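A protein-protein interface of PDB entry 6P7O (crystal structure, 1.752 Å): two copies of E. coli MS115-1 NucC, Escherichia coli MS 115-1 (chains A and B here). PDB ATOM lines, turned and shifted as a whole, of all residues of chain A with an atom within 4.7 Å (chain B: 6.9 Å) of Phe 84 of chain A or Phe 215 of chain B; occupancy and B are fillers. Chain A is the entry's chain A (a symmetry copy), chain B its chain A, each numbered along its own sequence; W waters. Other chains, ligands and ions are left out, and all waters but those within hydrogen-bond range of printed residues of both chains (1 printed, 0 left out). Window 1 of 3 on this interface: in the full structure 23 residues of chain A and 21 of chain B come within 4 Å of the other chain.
Among the printed residues, merely in contact across the chains: Ser 82 of chain A with Pro 51 of chain B (3.6 Å), Pro 83 of chain A with Pro 51 of chain B (3.9 Å), Pro 83 of chain A with Ile 218 of chain B (3.4 Å), Phe 84 of chain A with Phe 215 of chain B (3.5 Å), Phe 86 of chain A with Leu 6 of chain B (3.8 Å), Phe 86 of chain A with Phe 10 of chain B (3.9 Å), Phe 86 of chain A with Leu 13 of chain B (3.95 Å), Ile 232 of chain A with Phe 215 of chain B (3.7 Å), Ile 232 of chain A with Ala 219 of chain B (3.7 Å), Tyr 235 of chain A with Phe 10 of chain B (3.3 Å), Leu 239 of chain A with Phe 10 of chain B (3.4 Å), Leu 239 of chain A with Thr 211 of chain B (3.7 Å) and Leu 239 of chain A with Ala 212 of chain B (3.6 Å).
No position is printed for both chains.
Phe 84 of chain A touches one residue of chain B.
Phe 215 of chain B touches two residues of chain A.
Printed residues of chain B within 4 Å of Leu 239 of chain A: Phe 10 (3.4 Å), Thr 211 (3.7 Å) and Ala 212 (3.6 Å).
Printed residues of chain B within 4 Å of Phe 86 of chain A: Leu 6 (3.8 Å), Phe 10 (3.9 Å) and Leu 13 (3.95 Å).
Of the printed residues of chain A, Leu 6 of chain B touches Phe 86.
Of the printed residues of chain A, Leu 13 of chain B touches Phe 86 (3.95 Å).
Leu 214 of chain B touches none of the printed residues of chain A.
Gly 236 of chain A touches none of the printed residues of chain B.
The nearest residue of chain B that does not touch Phe 84 of chain A is Ile 218 of chain B (5.4 Å).
The nearest residue of chain A that does not touch Phe 215 of chain B is Gly 236 of chain A (4.5 Å).
Of the 10 printed residues of chain A, 7 touch a printed residue of chain B.
Hydrophobic or aromatic side chains of chain A within 4 Å of the printed part of chain B: Pro 83, Phe 84, Phe 86, Ile 232 and Leu 239.
Hydrophobic or aromatic side chains of chain B within 4 Å of the printed part of chain A: Leu 6, Phe 10, Leu 13, Pro 51, Ala 212, Phe 215, Ile 218 and Ala 219.
Among the printed residues, 13 pairs touch across the chains.
Water W1 bridges the backbone carbonyl oxygen of Tyr 49 of chain B and the backbone carbonyl oxygen of Pro 83 of chain A.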
ATOM      1  N   SER A  82      23.136 -10.422   9.860  1.00  0.00           N
ATOM      2  CA  SER A  82      23.455 -10.656   8.447  1.00  0.00           C
ATOM      3  C   SER A  82      23.394  -9.294   7.739  1.00  0.00           C
ATOM      4  O   SER A  82      22.440  -8.540   7.929  1.00  0.00           O
ATOM      5  CB  SER A  82      22.512 -11.614   7.745  1.00  0.00           C
ATOM      6  OG  SER A  82      22.544 -12.942   8.258  1.00  0.00           O
ATOM      7  N   PRO A  83      24.349  -8.988   6.872  1.00  0.00           N
ATOM      8  CA  PRO A  83      24.368  -7.672   6.215  1.00  0.00           C
ATOM      9  C   PRO A  83      23.314  -7.541   5.115  1.00  0.00           C
ATOM     10  O   PRO A  83      22.836  -6.441   4.844  1.00  0.00           O
ATOM     11  CB  PRO A  83      25.790  -7.590   5.616  1.00  0.00           C
ATOM     12  CG  PRO A  83      26.137  -9.084   5.330  1.00  0.00           C
ATOM     13  CD  PRO A  83      25.498  -9.820   6.523  1.00  0.00           C
ATOM     14  N   PHE A  84      22.931  -8.651   4.491  1.00  0.00           N
ATOM     15  CA  PHE A  84      21.904  -8.636   3.451  1.00  0.00           C
ATOM     16  C   PHE A  84      21.361 -10.038   3.259  1.00  0.00           C
ATOM     17  O   PHE A  84      21.978 -11.038   3.656  1.00  0.00           O
ATOM     18  CB  PHE A  84      22.468  -8.026   2.126  1.00  0.00           C
ATOM     19  CG  PHE A  84      23.762  -8.663   1.684  1.00  0.00           C
ATOM     20  CD1 PHE A  84      23.753  -9.801   0.937  1.00  0.00           C
ATOM     21  CD2 PHE A  84      24.954  -8.104   2.057  1.00  0.00           C
ATOM     22  CE1 PHE A  84      24.916 -10.453   0.576  1.00  0.00           C
ATOM     23  CE2 PHE A  84      26.116  -8.682   1.709  1.00  0.00           C
ATOM     24  CZ  PHE A  84      26.092  -9.929   0.931  1.00  0.00           C
ATOM     25  N   ILE A  85      20.144 -10.084   2.707  1.00  0.00           N
ATOM     26  CA  ILE A  85      19.508 -11.364   2.345  1.00  0.00           C
ATOM     27  C   ILE A  85      18.807 -11.096   1.026  1.00  0.00           C
ATOM     28  O   ILE A  85      17.811 -10.352   1.016  1.00  0.00           O
ATOM     29  CB  ILE A  85      18.482 -11.836   3.379  1.00  0.00           C
ATOM     30  CG1 ILE A  85      19.054 -11.986   4.797  1.00  0.00           C
ATOM     31  CG2 ILE A  85      17.851 -13.112   2.893  1.00  0.00           C
ATOM     32  CD1 ILE A  85      20.224 -12.997   4.971  1.00  0.00           C
ATOM     33  N   PHE A  86      19.327 -11.654  -0.092  1.00  0.00           N
ATOM     34  CA  PHE A  86      18.721 -11.384  -1.396  1.00  0.00           C
ATOM     35  C   PHE A  86      17.422 -12.171  -1.517  1.00  0.00           C
ATOM     36  O   PHE A  86      17.389 -13.361  -1.126  1.00  0.00           O
ATOM     37  CB  PHE A  86      19.650 -11.771  -2.569  1.00  0.00           C
ATOM     38  CG  PHE A  86      20.865 -10.869  -2.719  1.00  0.00           C
ATOM     39  CD1 PHE A  86      20.736  -9.588  -3.103  1.00  0.00           C
ATOM     40  CD2 PHE A  86      22.106 -11.384  -2.490  1.00  0.00           C
ATOM     41  CE1 PHE A  86      21.847  -8.773  -3.248  1.00  0.00           C
ATOM     42  CE2 PHE A  86      23.203 -10.610  -2.563  1.00  0.00           C
ATOM     43  CZ  PHE A  86      23.080  -9.316  -2.981  1.00  0.00           C
ATOM     44  N   PRO A  95      24.555 -14.500   2.370  1.00  0.00           N
ATOM     45  CA  PRO A  95      26.025 -14.504   2.250  1.00  0.00           C
ATOM     46  C   PRO A  95      26.641 -15.576   3.140  1.00  0.00           C
ATOM     47  O   PRO A  95      26.178 -15.868   4.249  1.00  0.00           O
ATOM     48  CB  PRO A  95      26.410 -13.083   2.702  1.00  0.00           C
ATOM     49  CG  PRO A  95      25.202 -12.710   3.668  1.00  0.00           C
ATOM     50  CD  PRO A  95      24.024 -13.284   3.056  1.00  0.00           C
ATOM     51  N   ILE A 232      32.240  -6.316   2.931  1.00  0.00           N
ATOM     52  CA  ILE A 232      31.035  -5.849   2.230  1.00  0.00           C
ATOM     53  C   ILE A 232      31.399  -5.141   0.936  1.00  0.00           C
ATOM     54  O   ILE A 232      30.703  -5.282  -0.098  1.00  0.00           O
ATOM     55  CB  ILE A 232      30.230  -4.909   3.166  1.00  0.00           C
ATOM     56  CG1 ILE A 232      29.826  -5.627   4.470  1.00  0.00           C
ATOM     57  CG2 ILE A 232      29.017  -4.314   2.498  1.00  0.00           C
ATOM     58  CD1 ILE A 232      28.985  -6.765   4.281  1.00  0.00           C
ATOM     59  N   TYR A 235      31.685  -7.582  -1.838  1.00  0.00           N
ATOM     60  CA  TYR A 235      30.363  -7.882  -2.398  1.00  0.00           C
ATOM     61  C   TYR A 235      29.866  -6.737  -3.284  1.00  0.00           C
ATOM     62  O   TYR A 235      29.360  -6.942  -4.384  1.00  0.00           O
ATOM     63  CB  TYR A 235      29.361  -8.175  -1.285  1.00  0.00           C
ATOM     64  CG  TYR A 235      29.418  -9.555  -0.735  1.00  0.00           C
ATOM     65  CD1 TYR A 235      28.826 -10.613  -1.402  1.00  0.00           C
ATOM     66  CD2 TYR A 235      29.983  -9.805   0.486  1.00  0.00           C
ATOM     67  CE1 TYR A 235      28.810 -11.911  -0.870  1.00  0.00           C
ATOM     68  CE2 TYR A 235      30.037 -11.052   0.994  1.00  0.00           C
ATOM     69  CZ  TYR A 235      29.420 -12.124   0.354  1.00  0.00           C
ATOM     70  OH  TYR A 235      29.422 -13.375   0.916  1.00  0.00           O
ATOM     71  N   GLY A 236      30.027  -5.522  -2.836  1.00  0.00           N
ATOM     72  CA  GLY A 236      29.523  -4.417  -3.578  1.00  0.00           C
ATOM     73  C   GLY A 236      30.160  -4.151  -4.915  1.00  0.00           C
ATOM     74  O   GLY A 236      29.627  -3.321  -5.679  1.00  0.00           O
ATOM     75  N   LEU A 239      27.976  -4.537  -7.892  1.00  0.00           N
ATOM     76  CA  LEU A 239      26.980  -3.574  -8.300  1.00  0.00           C
ATOM     77  C   LEU A 239      27.230  -3.030  -9.708  1.00  0.00           C
ATOM     78  O   LEU A 239      26.335  -2.410 -10.284  1.00  0.00           O
ATOM     79  CB  LEU A 239      26.978  -2.356  -7.381  1.00  0.00           C
ATOM     80  CG  LEU A 239      26.198  -2.611  -6.063  1.00  0.00           C
ATOM     81  CD1 LEU A 239      26.716  -1.583  -5.047  1.00  0.00           C
ATOM     82  CD2 LEU A 239      24.722  -2.546  -6.253  1.00  0.00           C
ATOM     83  N   LEU B   6      25.743 -12.975  -9.332  1.00  0.00           N
ATOM     84  CA  LEU B   6      25.608 -12.056  -8.226  1.00  0.00           C
ATOM     85  C   LEU B   6      25.279 -10.663  -8.730  1.00  0.00           C
ATOM     86  O   LEU B   6      24.556  -9.906  -8.081  1.00  0.00           O
ATOM     87  CB  LEU B   6      26.872 -12.096  -7.400  1.00  0.00           C
ATOM     88  CG  LEU B   6      26.952 -11.219  -6.193  1.00  0.00           C
ATOM     89  CD1 LEU B   6      25.743 -11.420  -5.201  1.00  0.00           C
ATOM     90  CD2 LEU B   6      28.244 -11.529  -5.479  1.00  0.00           C
ATOM     91  N   PHE B  10      22.057  -8.141  -7.510  1.00  0.00           N
ATOM     92  CA  PHE B  10      22.142  -6.738  -7.121  1.00  0.00           C
ATOM     93  C   PHE B  10      21.215  -5.867  -8.001  1.00  0.00           C
ATOM     94  O   PHE B  10      20.606  -4.888  -7.522  1.00  0.00           O
ATOM     95  CB  PHE B  10      23.614  -6.242  -7.243  1.00  0.00           C
ATOM     96  CG  PHE B  10      24.446  -6.450  -5.974  1.00  0.00           C
ATOM     97  CD1 PHE B  10      24.224  -5.623  -4.882  1.00  0.00           C
ATOM     98  CD2 PHE B  10      25.439  -7.408  -5.931  1.00  0.00           C
ATOM     99  CE1 PHE B  10      24.937  -5.765  -3.729  1.00  0.00           C
ATOM    100  CE2 PHE B  10      26.183  -7.585  -4.735  1.00  0.00           C
ATOM    101  CZ  PHE B  10      25.924  -6.727  -3.656  1.00  0.00           C
ATOM    102  N   LEU B  13      17.740  -6.386  -6.670  1.00  0.00           N
ATOM    103  CA  LEU B  13      17.553  -5.627  -5.449  1.00  0.00           C
ATOM    104  C   LEU B  13      17.369  -4.137  -5.741  1.00  0.00           C
ATOM    105  O   LEU B  13      16.518  -3.484  -5.115  1.00  0.00           O
ATOM    106  CB  LEU B  13      18.720  -5.852  -4.487  1.00  0.00           C
ATOM    107  CG  LEU B  13      18.860  -4.912  -3.276  1.00  0.00           C
ATOM    108  CD1 LEU B  13      17.689  -5.100  -2.305  1.00  0.00           C
ATOM    109  CD2 LEU B  13      20.203  -5.242  -2.589  1.00  0.00           C
ATOM    110  N   ILE B  17      14.330  -1.622  -4.720  1.00  0.00           N
ATOM    111  CA  ILE B  17      14.515  -0.400  -3.943  1.00  0.00           C
ATOM    112  C   ILE B  17      13.968   0.798  -4.700  1.00  0.00           C
ATOM    113  O   ILE B  17      13.363   1.690  -4.122  1.00  0.00           O
ATOM    114  CB  ILE B  17      15.997  -0.229  -3.610  1.00  0.00           C
ATOM    115  CG1 ILE B  17      16.331  -1.149  -2.435  1.00  0.00           C
ATOM    116  CG2 ILE B  17      16.347   1.256  -3.262  1.00  0.00           C
ATOM    117  CD1 ILE B  17      17.781  -1.229  -2.103  1.00  0.00           C
ATOM    118  N   TYR B  49      15.823  -2.784   4.664  1.00  0.00           N
ATOM    119  CA  TYR B  49      17.029  -3.439   4.177  1.00  0.00           C
ATOM    120  C   TYR B  49      18.236  -3.311   5.094  1.00  0.00           C
ATOM    121  O   TYR B  49      19.197  -4.023   4.869  1.00  0.00           O
ATOM    122  CB  TYR B  49      17.426  -2.876   2.775  1.00  0.00           C
ATOM    123  CG  TYR B  49      16.479  -3.362   1.708  1.00  0.00           C
ATOM    124  CD1 TYR B  49      16.541  -4.636   1.265  1.00  0.00           C
ATOM    125  CD2 TYR B  49      15.512  -2.534   1.179  1.00  0.00           C
ATOM    126  CE1 TYR B  49      15.673  -5.149   0.320  1.00  0.00           C
ATOM    127  CE2 TYR B  49      14.637  -3.014   0.214  1.00  0.00           C
ATOM    128  CZ  TYR B  49      14.718  -4.321  -0.214  1.00  0.00           C
ATOM    129  OH  TYR B  49      13.865  -4.867  -1.199  1.00  0.00           O
ATOM    130  N   PRO B  51      20.426  -4.298   8.331  1.00  0.00           N
ATOM    131  CA  PRO B  51      20.397  -5.408   9.296  1.00  0.00           C
ATOM    132  C   PRO B  51      19.463  -5.068  10.448  1.00  0.00           C
ATOM    133  O   PRO B  51      19.394  -3.924  10.890  1.00  0.00           O
ATOM    134  CB  PRO B  51      21.863  -5.512   9.761  1.00  0.00           C
ATOM    135  CG  PRO B  51      22.661  -4.991   8.543  1.00  0.00           C
ATOM    136  CD  PRO B  51      21.794  -3.852   7.994  1.00  0.00           C
ATOM    137  N   HIS B 191      26.399   8.165  -5.648  1.00  0.00           N
ATOM    138  CA  HIS B 191      26.530   8.361  -4.211  1.00  0.00           C
ATOM    139  C   HIS B 191      27.899   8.935  -3.917  1.00  0.00           C
ATOM    140  O   HIS B 191      28.783   8.999  -4.790  1.00  0.00           O
ATOM    141  CB  HIS B 191      26.182   7.055  -3.438  1.00  0.00           C
ATOM    142  CG  HIS B 191      27.306   6.061  -3.336  1.00  0.00           C
ATOM    143  ND1 HIS B 191      27.640   5.201  -4.353  1.00  0.00           N
ATOM    144  CD2 HIS B 191      28.112   5.733  -2.286  1.00  0.00           C
ATOM    145  CE1 HIS B 191      28.691   4.471  -3.977  1.00  0.00           C
ATOM    146  NE2 HIS B 191      28.975   4.764  -2.715  1.00  0.00           N
ATOM    147  N   PRO B 209      22.237   3.837  -7.766  1.00  0.00           N
ATOM    148  CA  PRO B 209      22.755   4.706  -6.695  1.00  0.00           C
ATOM    149  C   PRO B 209      22.290   4.373  -5.279  1.00  0.00           C
ATOM    150  O   PRO B 209      23.076   4.351  -4.326  1.00  0.00           O
ATOM    151  CB  PRO B 209      22.293   6.125  -7.172  1.00  0.00           C
ATOM    152  CG  PRO B 209      22.373   6.007  -8.719  1.00  0.00           C
ATOM    153  CD  PRO B 209      21.747   4.598  -8.962  1.00  0.00           C
ATOM    154  N   ALA B 210      21.008   4.156  -5.111  1.00  0.00           N
ATOM    155  CA  ALA B 210      20.502   3.977  -3.770  1.00  0.00           C
ATOM    156  C   ALA B 210      21.023   2.685  -3.175  1.00  0.00           C
ATOM    157  O   ALA B 210      21.183   2.580  -1.940  1.00  0.00           O
ATOM    158  CB  ALA B 210      18.988   3.942  -3.821  1.00  0.00           C
ATOM    159  N   THR B 211      21.163   1.677  -4.022  1.00  0.00           N
ATOM    160  CA  THR B 211      21.677   0.380  -3.563  1.00  0.00           C
ATOM    161  C   THR B 211      23.164   0.485  -3.272  1.00  0.00           C
ATOM    162  O   THR B 211      23.673  -0.062  -2.277  1.00  0.00           O
ATOM    163  CB  THR B 211      21.369  -0.699  -4.613  1.00  0.00           C
ATOM    164  OG1 THR B 211      19.939  -0.744  -4.814  1.00  0.00           O
ATOM    165  CG2 THR B 211      21.779  -2.086  -4.047  1.00  0.00           C
ATOM    166  N   ALA B 212      23.897   1.235  -4.102  1.00  0.00           N
ATOM    167  CA  ALA B 212      25.307   1.425  -3.794  1.00  0.00           C
ATOM    168  C   ALA B 212      25.495   2.192  -2.493  1.00  0.00           C
ATOM    169  O   ALA B 212      26.433   1.922  -1.718  1.00  0.00           O
ATOM    170  CB  ALA B 212      25.975   2.167  -4.932  1.00  0.00           C
ATOM    171  N   PHE B 213      24.646   3.184  -2.266  1.00  0.00           N
ATOM    172  CA  PHE B 213      24.641   3.923  -1.010  1.00  0.00           C
ATOM    173  C   PHE B 213      24.351   2.978   0.148  1.00  0.00           C
ATOM    174  O   PHE B 213      25.043   3.008   1.190  1.00  0.00           O
ATOM    175  CB  PHE B 213      23.590   5.080  -1.068  1.00  0.00           C
ATOM    176  CG  PHE B 213      23.207   5.579   0.305  1.00  0.00           C
ATOM    177  CD1 PHE B 213      24.110   6.340   1.056  1.00  0.00           C
ATOM    178  CD2 PHE B 213      22.024   5.170   0.868  1.00  0.00           C
ATOM    179  CE1 PHE B 213      23.782   6.663   2.363  1.00  0.00           C
ATOM    180  CE2 PHE B 213      21.710   5.481   2.195  1.00  0.00           C
ATOM    181  CZ  PHE B 213      22.596   6.203   2.920  1.00  0.00           C
ATOM    182  N   LEU B 214      23.317   2.146  -0.006  1.00  0.00           N
ATOM    183  CA  LEU B 214      22.977   1.194   1.070  1.00  0.00           C
ATOM    184  C   LEU B 214      24.182   0.326   1.440  1.00  0.00           C
ATOM    185  O   LEU B 214      24.489   0.137   2.624  1.00  0.00           O
ATOM    186  CB  LEU B 214      21.817   0.357   0.638  1.00  0.00           C
ATOM    187  CG  LEU B 214      21.390  -0.784   1.589  1.00  0.00           C
ATOM    188  CD1 LEU B 214      20.839  -0.379   2.861  1.00  0.00           C
ATOM    189  CD2 LEU B 214      20.458  -1.733   0.851  1.00  0.00           C
ATOM    190  N   PHE B 215      24.890  -0.188   0.440  1.00  0.00           N
ATOM    191  CA  PHE B 215      26.044  -1.035   0.712  1.00  0.00           C
ATOM    192  C   PHE B 215      27.215  -0.256   1.332  1.00  0.00           C
ATOM    193  O   PHE B 215      27.985  -0.818   2.137  1.00  0.00           O
ATOM    194  CB  PHE B 215      26.461  -1.829  -0.516  1.00  0.00           C
ATOM    195  CG  PHE B 215      25.720  -3.140  -0.564  1.00  0.00           C
ATOM    196  CD1 PHE B 215      24.330  -3.149  -0.673  1.00  0.00           C
ATOM    197  CD2 PHE B 215      26.381  -4.296  -0.349  1.00  0.00           C
ATOM    198  CE1 PHE B 215      23.615  -4.307  -0.604  1.00  0.00           C
ATOM    199  CE2 PHE B 215      25.660  -5.568  -0.260  1.00  0.00           C
ATOM    200  CZ  PHE B 215      24.289  -5.533  -0.388  1.00  0.00           C
ATOM    201  N   ARG B 216      27.364   1.012   1.003  1.00  0.00           N
ATOM    202  CA  ARG B 216      28.385   1.815   1.678  1.00  0.00           C
ATOM    203  C   ARG B 216      28.042   1.970   3.155  1.00  0.00           C
ATOM    204  O   ARG B 216      28.915   1.833   4.024  1.00  0.00           O
ATOM    205  CB  ARG B 216      28.492   3.187   1.000  1.00  0.00           C
ATOM    206  CG  ARG B 216      29.688   3.998   1.503  1.00  0.00           C
ATOM    207  CD  ARG B 216      30.947   3.413   0.869  1.00  0.00           C
ATOM    208  NE  ARG B 216      30.778   3.212  -0.585  1.00  0.00           N
ATOM    209  CZ  ARG B 216      31.585   2.487  -1.314  1.00  0.00           C
ATOM    210  NH1 ARG B 216      32.652   1.893  -0.748  1.00  0.00           N
ATOM    211  NH2 ARG B 216      31.353   2.384  -2.585  1.00  0.00           N
ATOM    212  N   LEU B 217      26.770   2.218   3.442  1.00  0.00           N
ATOM    213  CA  LEU B 217      26.329   2.415   4.798  1.00  0.00           C
ATOM    214  C   LEU B 217      26.483   1.135   5.576  1.00  0.00           C
ATOM    215  O   LEU B 217      26.990   1.146   6.711  1.00  0.00           O
ATOM    216  CB  LEU B 217      24.879   2.837   4.790  1.00  0.00           C
ATOM    217  CG  LEU B 217      24.178   3.039   6.143  1.00  0.00           C
ATOM    218  CD1 LEU B 217      24.953   3.973   7.059  1.00  0.00           C
ATOM    219  CD2 LEU B 217      22.740   3.536   5.918  1.00  0.00           C
ATOM    220  N   ILE B 218      26.040   0.011   5.016  1.00  0.00           N
ATOM    221  CA  ILE B 218      26.152  -1.241   5.789  1.00  0.00           C
ATOM    222  C   ILE B 218      27.611  -1.578   6.054  1.00  0.00           C
ATOM    223  O   ILE B 218      27.970  -2.064   7.127  1.00  0.00           O
ATOM    224  CB  ILE B 218      25.444  -2.386   5.032  1.00  0.00           C
ATOM    225  CG1 ILE B 218      23.957  -2.075   5.068  1.00  0.00           C
ATOM    226  CG2 ILE B 218      25.837  -3.732   5.562  1.00  0.00           C
ATOM    227  CD1 ILE B 218      23.191  -3.105   4.114  1.00  0.00           C
ATOM    228  N   ALA B 219      28.485  -1.346   5.077  1.00  0.00           N
ATOM    229  CA  ALA B 219      29.898  -1.636   5.281  1.00  0.00           C
ATOM    230  C   ALA B 219      30.479  -0.806   6.432  1.00  0.00           C
ATOM    231  O   ALA B 219      31.323  -1.290   7.182  1.00  0.00           O
ATOM    232  CB  ALA B 219      30.745  -1.355   4.000  1.00  0.00           C
ATOM    233  N   GLN B 220      30.096   0.464   6.515  1.00  0.00           N
ATOM    234  CA  GLN B 220      30.649   1.305   7.568  1.00  0.00           C
ATOM    235  C   GLN B 220      30.008   0.980   8.923  1.00  0.00           C
ATOM    236  O   GLN B 220      30.684   0.980   9.945  1.00  0.00           O
ATOM    237  CB  GLN B 220      30.472   2.772   7.208  1.00  0.00           C
ATOM    238  CG  GLN B 220      31.214   3.718   8.054  1.00  0.00           C
ATOM    239  CD  GLN B 220      32.672   3.529   7.933  1.00  0.00           C
ATOM    240  OE1 GLN B 220      33.236   3.608   6.820  1.00  0.00           O
ATOM    241  NE2 GLN B 220      33.318   3.219   9.073  1.00  0.00           N
HETATM  242  O   HOH W   1      20.697  -5.394   3.141  1.00  0.00           O
